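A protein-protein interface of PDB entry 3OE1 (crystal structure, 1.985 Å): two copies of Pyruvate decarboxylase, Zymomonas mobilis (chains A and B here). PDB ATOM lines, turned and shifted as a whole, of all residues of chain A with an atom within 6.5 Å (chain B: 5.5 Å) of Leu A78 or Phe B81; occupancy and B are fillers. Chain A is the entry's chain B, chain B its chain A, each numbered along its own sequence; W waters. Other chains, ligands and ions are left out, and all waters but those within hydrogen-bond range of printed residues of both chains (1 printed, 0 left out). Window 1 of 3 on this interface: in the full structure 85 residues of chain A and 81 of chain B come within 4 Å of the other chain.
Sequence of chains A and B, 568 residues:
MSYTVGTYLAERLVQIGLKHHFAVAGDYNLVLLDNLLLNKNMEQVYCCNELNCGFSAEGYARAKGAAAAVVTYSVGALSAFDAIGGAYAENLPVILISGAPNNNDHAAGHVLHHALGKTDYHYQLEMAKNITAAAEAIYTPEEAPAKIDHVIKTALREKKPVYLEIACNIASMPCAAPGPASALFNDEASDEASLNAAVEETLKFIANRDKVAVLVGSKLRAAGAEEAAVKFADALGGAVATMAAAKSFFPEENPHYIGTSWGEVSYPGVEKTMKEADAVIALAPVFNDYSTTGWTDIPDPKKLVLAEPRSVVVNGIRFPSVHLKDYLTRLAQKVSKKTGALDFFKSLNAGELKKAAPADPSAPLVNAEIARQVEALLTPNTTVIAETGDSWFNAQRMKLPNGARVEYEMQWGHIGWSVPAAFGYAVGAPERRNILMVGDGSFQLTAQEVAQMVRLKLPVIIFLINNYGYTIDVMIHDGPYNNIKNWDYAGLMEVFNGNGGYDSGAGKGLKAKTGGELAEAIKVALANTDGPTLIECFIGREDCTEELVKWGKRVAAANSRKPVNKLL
Of the 17 printed residues of chain A, 8 touch a printed residue of chain B. Hydrophobic or aromatic side chains of chain A within 4 Å of the printed part of chain B: Val A75, Leu A78, Leu A116 and Met A127. Of the 18 printed residues of chain B, 7 touch a printed residue of chain A. Printed residues of chain B that touch a printed residue of chain A: Leu B78, Ser B79, Phe B81, Asp B82, Gly B85, Met B127 and Trp B412. Among the printed residues, no Asp or Glu carboxylate lies within 4 Å of a Lys or Arg side-chain nitrogen of the other chain.
The backbone carbonyl oxygen (O) of Gly B76 sits at hydrogen-bond distance from the side-chain hydroxyl (OG) of Ser B79. O of Asp B82 sits at hydrogen-bond distance from NE1 of Trp B412 (2.9 Å). The side-chain hydroxyl (OG) of Ser A74 is in hydrogen-bond range of the side-chain hydroxyl (OH) of Tyr A123. NE2 of Gln A124 sits close to N of Ser A74 (2.8 Å). O of Gly A76 sits at hydrogen-bond distance from OG of Ser A79 (3.4 Å).
Water W1 lies within hydrogen-bond range of the backbone carbonyl oxygen (O) of Leu B78 and the backbone carbonyl oxygen (O) of Leu A78.
Leu A78 touches its own counterpart, Leu B78. Leu A78 touches Phe B81, and with the chains exchanged Phe A81 touches Leu B78. Leu A78 touches Asp B82, and with the chains exchanged Asp A82 touches Leu B78. Met B127 touches its own counterpart, Met A127. Positions printed for both chains: 76, 77, 78, 79, 80, 81, 82, 83, 124 and 127.
The backbone NH (N) of Ser B79 sits close to the side-chain carboxylate (OD2) of Asp A82. The side-chain carboxylate (OD2) of Asp B82 sits close to the backbone carbonyl oxygen (O) of Val A75. OD2 of Asp B82 lies within hydrogen-bond range of N of Ser A79, 3.3 Å away. The backbone carbonyl oxygen (O) of Leu A78 sits close to the backbone carbonyl oxygen (O) of Leu B78 (3.4 Å).
Leu A78 touches just these residues of chain B: Leu B78 (3.4 Å), Phe B81 (3.8 Å) and Asp B82 (3.8 Å). Of the printed residues of chain B, Phe A81 touches Leu B78. Of the printed residues of chain B, Asp A82 touches Leu B78 (3.9 Å) and Ser B79 (3.3 Å). Printed residues of chain A within 4 Å of Leu B78: Leu A78, Phe A81 and Asp A82. Of the printed residues of chain A, Phe B81 touches Leu A78 (3.8 Å). Printed residues of chain A within 4 Å of Asp B82: Ser A74 (3.99 Å), Val A75 (2.7 Å), Leu A78 (3.8 Å) and Ser A79 (3.3 Å). Ala B128 touches none of the printed residues of chain A. The nearest residue of chain B that does not touch Leu A78 is Trp B412 (4.1 Å). The nearest residue of chain A that does not touch Phe B81 is Met A127 (4.2 Å). The nearest printed residue of chain A that does not touch Ser B79 is Ser A79 (4.3 Å).
Among the printed residues, merely in contact across the chains: Ser A74 with Asp B82 (3.99 Å), Ser A74 with Trp B412 (3.0 Å), Val A75 with Trp B412 (3.0 Å), Leu A78 with Phe B81 (3.8 Å), Leu A78 with Asp B82 (3.8 Å), Phe A81 with Leu B78 (3.96 Å), Asp A82 with Leu B78 (3.9 Å), Leu A116 with Gly B85 (3.9 Å), Leu A116 with Trp B412 (3.9 Å) and Met A127 with Met B127 (3.8 Å).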
ATOM      1  N   VAL A  71      26.715 -35.867  30.372  1.00  0.00           N
ATOM      2  CA  VAL A  71      26.194 -35.012  31.433  1.00  0.00           C
ATOM      3  C   VAL A  71      24.783 -35.460  31.823  1.00  0.00           C
ATOM      4  O   VAL A  71      24.255 -36.416  31.256  1.00  0.00           O
ATOM      5  CB  VAL A  71      26.158 -33.532  30.995  1.00  0.00           C
ATOM      6  CG1 VAL A  71      27.537 -33.079  30.524  1.00  0.00           C
ATOM      7  CG2 VAL A  71      25.128 -33.328  29.889  1.00  0.00           C
ATOM      8  N   THR A  72      24.183 -34.789  32.803  1.00  0.00           N
ATOM      9  CA  THR A  72      22.815 -35.109  33.204  1.00  0.00           C
ATOM     10  C   THR A  72      21.823 -34.166  32.530  1.00  0.00           C
ATOM     11  O   THR A  72      22.210 -33.137  31.966  1.00  0.00           O
ATOM     12  CB  THR A  72      22.630 -35.070  34.736  1.00  0.00           C
ATOM     13  OG1 THR A  72      21.440 -35.778  35.090  1.00  0.00           O
ATOM     14  CG2 THR A  72      22.542 -33.637  35.241  1.00  0.00           C
ATOM     15  N   TYR A  73      20.545 -34.507  32.596  1.00  0.00           N
ATOM     16  CA  TYR A  73      19.542 -33.745  31.865  1.00  0.00           C
ATOM     17  C   TYR A  73      19.431 -32.297  32.340  1.00  0.00           C
ATOM     18  O   TYR A  73      19.212 -32.032  33.523  1.00  0.00           O
ATOM     19  CB  TYR A  73      18.170 -34.427  31.929  1.00  0.00           C
ATOM     20  CG  TYR A  73      17.190 -33.864  30.922  1.00  0.00           C
ATOM     21  CD1 TYR A  73      17.278 -34.204  29.579  1.00  0.00           C
ATOM     22  CD2 TYR A  73      16.188 -32.987  31.313  1.00  0.00           C
ATOM     23  CE1 TYR A  73      16.396 -33.682  28.653  1.00  0.00           C
ATOM     24  CE2 TYR A  73      15.296 -32.463  30.391  1.00  0.00           C
ATOM     25  CZ  TYR A  73      15.406 -32.816  29.064  1.00  0.00           C
ATOM     26  OH  TYR A  73      14.522 -32.296  28.141  1.00  0.00           O
ATOM     27  N   SER A  74      19.608 -31.369  31.402  1.00  0.00           N
ATOM     28  CA  SER A  74      19.192 -29.980  31.580  1.00  0.00           C
ATOM     29  C   SER A  74      20.168 -29.152  32.396  1.00  0.00           C
ATOM     30  O   SER A  74      20.865 -28.295  31.853  1.00  0.00           O
ATOM     31  CB  SER A  74      17.789 -29.913  32.186  1.00  0.00           C
ATOM     32  OG  SER A  74      17.208 -28.649  31.968  1.00  0.00           O
ATOM     33  N   VAL A  75      20.214 -29.399  33.698  1.00  0.00           N
ATOM     34  CA  VAL A  75      21.178 -28.709  34.537  1.00  0.00           C
ATOM     35  C   VAL A  75      22.590 -29.040  34.062  1.00  0.00           C
ATOM     36  O   VAL A  75      23.496 -28.213  34.153  1.00  0.00           O
ATOM     37  CB  VAL A  75      20.989 -29.025  36.039  1.00  0.00           C
ATOM     38  CG1 VAL A  75      19.595 -28.598  36.489  1.00  0.00           C
ATOM     39  CG2 VAL A  75      21.224 -30.507  36.328  1.00  0.00           C
ATOM     40  N   GLY A  76      22.770 -30.242  33.526  1.00  0.00           N
ATOM     41  CA  GLY A  76      24.065 -30.630  32.987  1.00  0.00           C
ATOM     42  C   GLY A  76      24.284 -30.200  31.539  1.00  0.00           C
ATOM     43  O   GLY A  76      25.350 -29.694  31.181  1.00  0.00           O
ATOM     44  N   ALA A  77      23.260 -30.380  30.713  1.00  0.00           N
ATOM     45  CA  ALA A  77      23.382 -30.186  29.272  1.00  0.00           C
ATOM     46  C   ALA A  77      23.500 -28.723  28.829  1.00  0.00           C
ATOM     47  O   ALA A  77      24.302 -28.402  27.957  1.00  0.00           O
ATOM     48  CB  ALA A  77      22.221 -30.852  28.560  1.00  0.00           C
ATOM     49  N   LEU A  78      22.694 -27.846  29.417  1.00  0.00           N
ATOM     50  CA  LEU A  78      22.618 -26.460  28.964  1.00  0.00           C
ATOM     51  C   LEU A  78      23.957 -25.713  29.036  1.00  0.00           C
ATOM     52  O   LEU A  78      24.311 -24.963  28.125  1.00  0.00           O
ATOM     53  CB  LEU A  78      21.519 -25.699  29.720  1.00  0.00           C
ATOM     54  CG  LEU A  78      20.169 -25.586  28.992  1.00  0.00           C
ATOM     55  CD1 LEU A  78      19.659 -26.953  28.559  1.00  0.00           C
ATOM     56  CD2 LEU A  78      19.113 -24.867  29.841  1.00  0.00           C
ATOM     57  N   SER A  79      24.706 -25.915  30.112  1.00  0.00           N
ATOM     58  CA  SER A  79      26.010 -25.272  30.219  1.00  0.00           C
ATOM     59  C   SER A  79      26.991 -25.910  29.238  1.00  0.00           C
ATOM     60  O   SER A  79      27.794 -25.219  28.613  1.00  0.00           O
ATOM     61  CB  SER A  79      26.539 -25.338  31.651  1.00  0.00           C
ATOM     62  OG  SER A  79      26.712 -26.677  32.059  1.00  0.00           O
ATOM     63  N   ALA A  80      26.897 -27.229  29.084  1.00  0.00           N
ATOM     64  CA  ALA A  80      27.743 -27.954  28.145  1.00  0.00           C
ATOM     65  C   ALA A  80      27.508 -27.486  26.707  1.00  0.00           C
ATOM     66  O   ALA A  80      28.414 -27.535  25.877  1.00  0.00           O
ATOM     67  CB  ALA A  80      27.513 -29.456  28.268  1.00  0.00           C
ATOM     68  N   PHE A  81      26.291 -27.025  26.428  1.00  0.00           N
ATOM     69  CA  PHE A  81      25.926 -26.556  25.098  1.00  0.00           C
ATOM     70  C   PHE A  81      26.894 -25.473  24.611  1.00  0.00           C
ATOM     71  O   PHE A  81      27.182 -25.371  23.419  1.00  0.00           O
ATOM     72  CB  PHE A  81      24.496 -26.009  25.089  1.00  0.00           C
ATOM     73  CG  PHE A  81      23.432 -27.061  24.926  1.00  0.00           C
ATOM     74  CD1 PHE A  81      23.765 -28.381  24.693  1.00  0.00           C
ATOM     75  CD2 PHE A  81      22.089 -26.715  24.990  1.00  0.00           C
ATOM     76  CE1 PHE A  81      22.775 -29.354  24.543  1.00  0.00           C
ATOM     77  CE2 PHE A  81      21.096 -27.674  24.832  1.00  0.00           C
ATOM     78  CZ  PHE A  81      21.440 -28.995  24.606  1.00  0.00           C
ATOM     79  N   ASP A  82      27.373 -24.660  25.547  1.00  0.00           N
ATOM     80  CA  ASP A  82      28.335 -23.611  25.248  1.00  0.00           C
ATOM     81  C   ASP A  82      29.590 -24.238  24.664  1.00  0.00           C
ATOM     82  O   ASP A  82      30.132 -23.759  23.663  1.00  0.00           O
ATOM     83  CB  ASP A  82      28.670 -22.845  26.527  1.00  0.00           C
ATOM     84  CG  ASP A  82      29.331 -21.513  26.259  1.00  0.00           C
ATOM     85  OD1 ASP A  82      29.894 -21.314  25.166  1.00  0.00           O
ATOM     86  OD2 ASP A  82      29.304 -20.657  27.159  1.00  0.00           O
ATOM     87  N   ALA A  83      30.038 -25.324  25.289  1.00  0.00           N
ATOM     88  CA  ALA A  83      31.229 -26.037  24.826  1.00  0.00           C
ATOM     89  C   ALA A  83      30.983 -26.732  23.478  1.00  0.00           C
ATOM     90  O   ALA A  83      31.865 -26.777  22.621  1.00  0.00           O
ATOM     91  CB  ALA A  83      31.693 -27.039  25.881  1.00  0.00           C
ATOM     92  N   LEU A 116      12.025 -27.365  33.529  1.00  0.00           N
ATOM     93  CA  LEU A 116      11.470 -26.015  33.571  1.00  0.00           C
ATOM     94  C   LEU A 116      10.231 -25.872  34.456  1.00  0.00           C
ATOM     95  O   LEU A 116       9.790 -24.758  34.746  1.00  0.00           O
ATOM     96  CB  LEU A 116      11.171 -25.533  32.144  1.00  0.00           C
ATOM     97  CG  LEU A 116      12.398 -25.382  31.245  1.00  0.00           C
ATOM     98  CD1 LEU A 116      12.006 -25.355  29.769  1.00  0.00           C
ATOM     99  CD2 LEU A 116      13.185 -24.129  31.612  1.00  0.00           C
ATOM    100  N   TYR A 123      12.531 -29.660  24.918  1.00  0.00           N
ATOM    101  CA  TYR A 123      13.174 -28.363  24.740  1.00  0.00           C
ATOM    102  C   TYR A 123      14.694 -28.498  24.617  1.00  0.00           C
ATOM    103  O   TYR A 123      15.317 -27.807  23.814  1.00  0.00           O
ATOM    104  CB  TYR A 123      12.791 -27.375  25.851  1.00  0.00           C
ATOM    105  CG  TYR A 123      13.323 -27.718  27.223  1.00  0.00           C
ATOM    106  CD1 TYR A 123      12.552 -28.438  28.123  1.00  0.00           C
ATOM    107  CD2 TYR A 123      14.594 -27.313  27.624  1.00  0.00           C
ATOM    108  CE1 TYR A 123      13.028 -28.755  29.381  1.00  0.00           C
ATOM    109  CE2 TYR A 123      15.083 -27.630  28.884  1.00  0.00           C
ATOM    110  CZ  TYR A 123      14.293 -28.351  29.757  1.00  0.00           C
ATOM    111  OH  TYR A 123      14.750 -28.675  31.016  1.00  0.00           O
ATOM    112  N   GLN A 124      15.287 -29.389  25.411  1.00  0.00           N
ATOM    113  CA  GLN A 124      16.732 -29.595  25.359  1.00  0.00           C
ATOM    114  C   GLN A 124      17.163 -30.082  23.979  1.00  0.00           C
ATOM    115  O   GLN A 124      18.104 -29.547  23.390  1.00  0.00           O
ATOM    116  CB  GLN A 124      17.186 -30.578  26.436  1.00  0.00           C
ATOM    117  CG  GLN A 124      18.663 -30.923  26.364  1.00  0.00           C
ATOM    118  CD  GLN A 124      19.149 -31.618  27.619  1.00  0.00           C
ATOM    119  OE1 GLN A 124      19.680 -32.736  27.572  1.00  0.00           O
ATOM    120  NE2 GLN A 124      18.966 -30.963  28.754  1.00  0.00           N
ATOM    121  N   MET A 127      16.965 -27.220  21.437  1.00  0.00           N
ATOM    122  CA  MET A 127      18.062 -26.277  21.581  1.00  0.00           C
ATOM    123  C   MET A 127      19.313 -26.878  20.956  1.00  0.00           C
ATOM    124  O   MET A 127      20.055 -26.197  20.248  1.00  0.00           O
ATOM    125  CB  MET A 127      18.303 -25.939  23.055  1.00  0.00           C
ATOM    126  CG  MET A 127      17.199 -25.088  23.692  1.00  0.00           C
ATOM    127  SD  MET A 127      17.331 -24.934  25.489  1.00  0.00           S
ATOM    128  CE  MET A 127      18.671 -23.749  25.674  1.00  0.00           C
ATOM    129  N   GLY B  76      29.098 -16.073  26.030  1.00  0.00           N
ATOM    130  CA  GLY B  76      28.533 -15.634  27.292  1.00  0.00           C
ATOM    131  C   GLY B  76      27.126 -16.151  27.557  1.00  0.00           C
ATOM    132  O   GLY B  76      26.842 -16.658  28.638  1.00  0.00           O
ATOM    133  N   ALA B  77      26.242 -16.022  26.571  1.00  0.00           N
ATOM    134  CA  ALA B  77      24.826 -16.347  26.759  1.00  0.00           C
ATOM    135  C   ALA B  77      24.520 -17.841  26.904  1.00  0.00           C
ATOM    136  O   ALA B  77      23.646 -18.229  27.679  1.00  0.00           O
ATOM    137  CB  ALA B  77      23.991 -15.748  25.631  1.00  0.00           C
ATOM    138  N   LEU B  78      25.218 -18.685  26.157  1.00  0.00           N
ATOM    139  CA  LEU B  78      24.852 -20.098  26.136  1.00  0.00           C
ATOM    140  C   LEU B  78      25.002 -20.768  27.496  1.00  0.00           C
ATOM    141  O   LEU B  78      24.145 -21.555  27.897  1.00  0.00           O
ATOM    142  CB  LEU B  78      25.597 -20.868  25.041  1.00  0.00           C
ATOM    143  CG  LEU B  78      24.733 -21.148  23.806  1.00  0.00           C
ATOM    144  CD1 LEU B  78      24.095 -19.850  23.300  1.00  0.00           C
ATOM    145  CD2 LEU B  78      25.534 -21.840  22.695  1.00  0.00           C
ATOM    146  N   SER B  79      26.073 -20.450  28.214  1.00  0.00           N
ATOM    147  CA  SER B  79      26.244 -20.992  29.557  1.00  0.00           C
ATOM    148  C   SER B  79      25.275 -20.314  30.525  1.00  0.00           C
ATOM    149  O   SER B  79      24.727 -20.962  31.418  1.00  0.00           O
ATOM    150  CB  SER B  79      27.687 -20.839  30.039  1.00  0.00           C
ATOM    151  OG  SER B  79      27.993 -19.484  30.289  1.00  0.00           O
ATOM    152  N   ALA B  80      25.054 -19.014  30.337  1.00  0.00           N
ATOM    153  CA  ALA B  80      24.078 -18.285  31.147  1.00  0.00           C
ATOM    154  C   ALA B  80      22.654 -18.828  30.988  1.00  0.00           C
ATOM    155  O   ALA B  80      21.833 -18.705  31.902  1.00  0.00           O
ATOM    156  CB  ALA B  80      24.115 -16.799  30.822  1.00  0.00           C
ATOM    157  N   PHE B  81      22.360 -19.413  29.828  1.00  0.00           N
ATOM    158  CA  PHE B  81      21.065 -20.064  29.603  1.00  0.00           C
ATOM    159  C   PHE B  81      20.749 -21.087  30.696  1.00  0.00           C
ATOM    160  O   PHE B  81      19.595 -21.259  31.077  1.00  0.00           O
ATOM    161  CB  PHE B  81      21.020 -20.777  28.244  1.00  0.00           C
ATOM    162  CG  PHE B  81      20.818 -19.862  27.065  1.00  0.00           C
ATOM    163  CD1 PHE B  81      21.025 -20.329  25.772  1.00  0.00           C
ATOM    164  CD2 PHE B  81      20.425 -18.545  27.240  1.00  0.00           C
ATOM    165  CE1 PHE B  81      20.845 -19.502  24.677  1.00  0.00           C
ATOM    166  CE2 PHE B  81      20.237 -17.713  26.147  1.00  0.00           C
ATOM    167  CZ  PHE B  81      20.447 -18.190  24.866  1.00  0.00           C
ATOM    168  N   ASP B  82      21.773 -21.780  31.188  1.00  0.00           N
ATOM    169  CA  ASP B  82      21.562 -22.803  32.213  1.00  0.00           C
ATOM    170  C   ASP B  82      20.984 -22.163  33.481  1.00  0.00           C
ATOM    171  O   ASP B  82      20.052 -22.688  34.096  1.00  0.00           O
ATOM    172  CB  ASP B  82      22.875 -23.540  32.509  1.00  0.00           C
ATOM    173  CG  ASP B  82      22.667 -24.834  33.288  1.00  0.00           C
ATOM    174  OD1 ASP B  82      21.620 -24.977  33.947  1.00  0.00           O
ATOM    175  OD2 ASP B  82      23.560 -25.711  33.249  1.00  0.00           O
ATOM    176  N   ALA B  83      21.538 -21.017  33.862  1.00  0.00           N
ATOM    177  CA  ALA B  83      21.035 -20.267  35.005  1.00  0.00           C
ATOM    178  C   ALA B  83      19.664 -19.669  34.693  1.00  0.00           C
ATOM    179  O   ALA B  83      18.777 -19.647  35.543  1.00  0.00           O
ATOM    180  CB  ALA B  83      22.013 -19.183  35.392  1.00  0.00           C
ATOM    181  N   ILE B  84      19.481 -19.204  33.464  1.00  0.00           N
ATOM    182  CA  ILE B  84      18.189 -18.649  33.065  1.00  0.00           C
ATOM    183  C   ILE B  84      17.090 -19.711  33.115  1.00  0.00           C
ATOM    184  O   ILE B  84      16.007 -19.473  33.652  1.00  0.00           O
ATOM    185  CB  ILE B  84      18.259 -18.002  31.680  1.00  0.00           C
ATOM    186  CG1 ILE B  84      19.154 -16.763  31.742  1.00  0.00           C
ATOM    187  CG2 ILE B  84      16.860 -17.656  31.176  1.00  0.00           C
ATOM    188  CD1 ILE B  84      18.756 -15.771  32.817  1.00  0.00           C
ATOM    189  N   GLY B  85      17.378 -20.881  32.554  1.00  0.00           N
ATOM    190  CA  GLY B  85      16.499 -22.023  32.708  1.00  0.00           C
ATOM    191  C   GLY B  85      16.172 -22.200  34.176  1.00  0.00           C
ATOM    192  O   GLY B  85      15.027 -22.435  34.541  1.00  0.00           O
ATOM    193  N   GLY B  86      17.191 -22.068  35.022  1.00  0.00           N
ATOM    194  CA  GLY B  86      17.017 -22.160  36.460  1.00  0.00           C
ATOM    195  C   GLY B  86      16.052 -21.131  37.034  1.00  0.00           C
ATOM    196  O   GLY B  86      15.230 -21.452  37.889  1.00  0.00           O
ATOM    197  N   LEU B  96      17.936 -11.440  31.265  1.00  0.00           N
ATOM    198  CA  LEU B  96      19.203 -11.694  30.603  1.00  0.00           C
ATOM    199  C   LEU B  96      19.334 -10.800  29.377  1.00  0.00           C
ATOM    200  O   LEU B  96      18.539 -10.886  28.443  1.00  0.00           O
ATOM    201  CB  LEU B  96      19.334 -13.169  30.202  1.00  0.00           C
ATOM    202  CG  LEU B  96      20.665 -13.570  29.555  1.00  0.00           C
ATOM    203  CD1 LEU B  96      21.827 -13.413  30.529  1.00  0.00           C
ATOM    204  CD2 LEU B  96      20.600 -15.004  29.026  1.00  0.00           C
ATOM    205  N   GLN B 124      20.795 -18.044  18.747  1.00  0.00           N
ATOM    206  CA  GLN B 124      20.774 -17.771  20.176  1.00  0.00           C
ATOM    207  C   GLN B 124      19.386 -17.307  20.614  1.00  0.00           C
ATOM    208  O   GLN B 124      18.863 -17.765  21.622  1.00  0.00           O
ATOM    209  CB  GLN B 124      21.847 -16.748  20.550  1.00  0.00           C
ATOM    210  CG  GLN B 124      21.867 -16.393  22.018  1.00  0.00           C
ATOM    211  CD  GLN B 124      23.013 -15.482  22.372  1.00  0.00           C
ATOM    212  OE1 GLN B 124      24.174 -15.874  22.288  1.00  0.00           O
ATOM    213  NE2 GLN B 124      22.696 -14.255  22.765  1.00  0.00           N
ATOM    214  N   MET B 127      17.147 -20.534  20.685  1.00  0.00           N
ATOM    215  CA  MET B 127      17.414 -21.365  21.843  1.00  0.00           C
ATOM    216  C   MET B 127      16.773 -20.733  23.077  1.00  0.00           C
ATOM    217  O   MET B 127      16.128 -21.413  23.879  1.00  0.00           O
ATOM    218  CB  MET B 127      18.924 -21.532  22.047  1.00  0.00           C
ATOM    219  CG  MET B 127      19.641 -22.175  20.883  1.00  0.00           C
ATOM    220  SD  MET B 127      21.415 -22.303  21.173  1.00  0.00           S
ATOM    221  CE  MET B 127      21.470 -23.491  22.512  1.00  0.00           C
ATOM    222  N   ALA B 128      16.937 -19.420  23.214  1.00  0.00           N
ATOM    223  CA  ALA B 128      16.462 -18.694  24.396  1.00  0.00           C
ATOM    224  C   ALA B 128      14.940 -18.691  24.563  1.00  0.00           C
ATOM    225  O   ALA B 128      14.440 -18.669  25.683  1.00  0.00           O
ATOM    226  CB  ALA B 128      17.000 -17.268  24.390  1.00  0.00           C
ATOM    227  N   ILE B 131      13.392 -21.178  27.145  1.00  0.00           N
ATOM    228  CA  ILE B 131      13.617 -21.121  28.584  1.00  0.00           C
ATOM    229  C   ILE B 131      13.262 -19.764  29.174  1.00  0.00           C
ATOM    230  O   ILE B 131      13.767 -19.388  30.229  1.00  0.00           O
ATOM    231  CB  ILE B 131      15.089 -21.468  28.911  1.00  0.00           C
ATOM    232  CG1 ILE B 131      16.031 -20.435  28.283  1.00  0.00           C
ATOM    233  CG2 ILE B 131      15.420 -22.856  28.393  1.00  0.00           C
ATOM    234  CD1 ILE B 131      17.489 -20.767  28.410  1.00  0.00           C
ATOM    235  N   TYR B 163      14.576 -12.556  27.978  1.00  0.00           N
ATOM    236  CA  TYR B 163      15.792 -12.487  27.187  1.00  0.00           C
ATOM    237  C   TYR B 163      15.765 -11.267  26.286  1.00  0.00           C
ATOM    238  O   TYR B 163      14.774 -11.010  25.605  1.00  0.00           O
ATOM    239  CB  TYR B 163      15.924 -13.750  26.331  1.00  0.00           C
ATOM    240  CG  TYR B 163      17.021 -13.696  25.291  1.00  0.00           C
ATOM    241  CD1 TYR B 163      18.322 -14.043  25.615  1.00  0.00           C
ATOM    242  CD2 TYR B 163      16.754 -13.309  23.979  1.00  0.00           C
ATOM    243  CE1 TYR B 163      19.328 -14.005  24.674  1.00  0.00           C
ATOM    244  CE2 TYR B 163      17.768 -13.262  23.024  1.00  0.00           C
ATOM    245  CZ  TYR B 163      19.056 -13.619  23.388  1.00  0.00           C
ATOM    246  OH  TYR B 163      20.093 -13.592  22.476  1.00  0.00           O
ATOM    247  N   TRP B 412      15.054 -26.722  39.747  1.00  0.00           N
ATOM    248  CA  TRP B 412      16.193 -26.825  38.845  1.00  0.00           C
ATOM    249  C   TRP B 412      17.230 -27.808  39.384  1.00  0.00           C
ATOM    250  O   TRP B 412      17.626 -28.744  38.695  1.00  0.00           O
ATOM    251  CB  TRP B 412      16.827 -25.453  38.632  1.00  0.00           C
ATOM    252  CG  TRP B 412      17.585 -25.318  37.345  1.00  0.00           C
ATOM    253  CD1 TRP B 412      18.872 -24.882  37.197  1.00  0.00           C
ATOM    254  CD2 TRP B 412      17.102 -25.596  36.019  1.00  0.00           C
ATOM    255  NE1 TRP B 412      19.221 -24.874  35.867  1.00  0.00           N
ATOM    256  CE2 TRP B 412      18.154 -25.304  35.122  1.00  0.00           C
ATOM    257  CE3 TRP B 412      15.883 -26.065  35.504  1.00  0.00           C
ATOM    258  CZ2 TRP B 412      18.031 -25.471  33.741  1.00  0.00           C
ATOM    259  CZ3 TRP B 412      15.759 -26.228  34.129  1.00  0.00           C
ATOM    260  CH2 TRP B 412      16.830 -25.928  33.262  1.00  0.00           C
HETATM  261  O   HOH W   1      22.813 -23.371  26.545  1.00  0.00           O
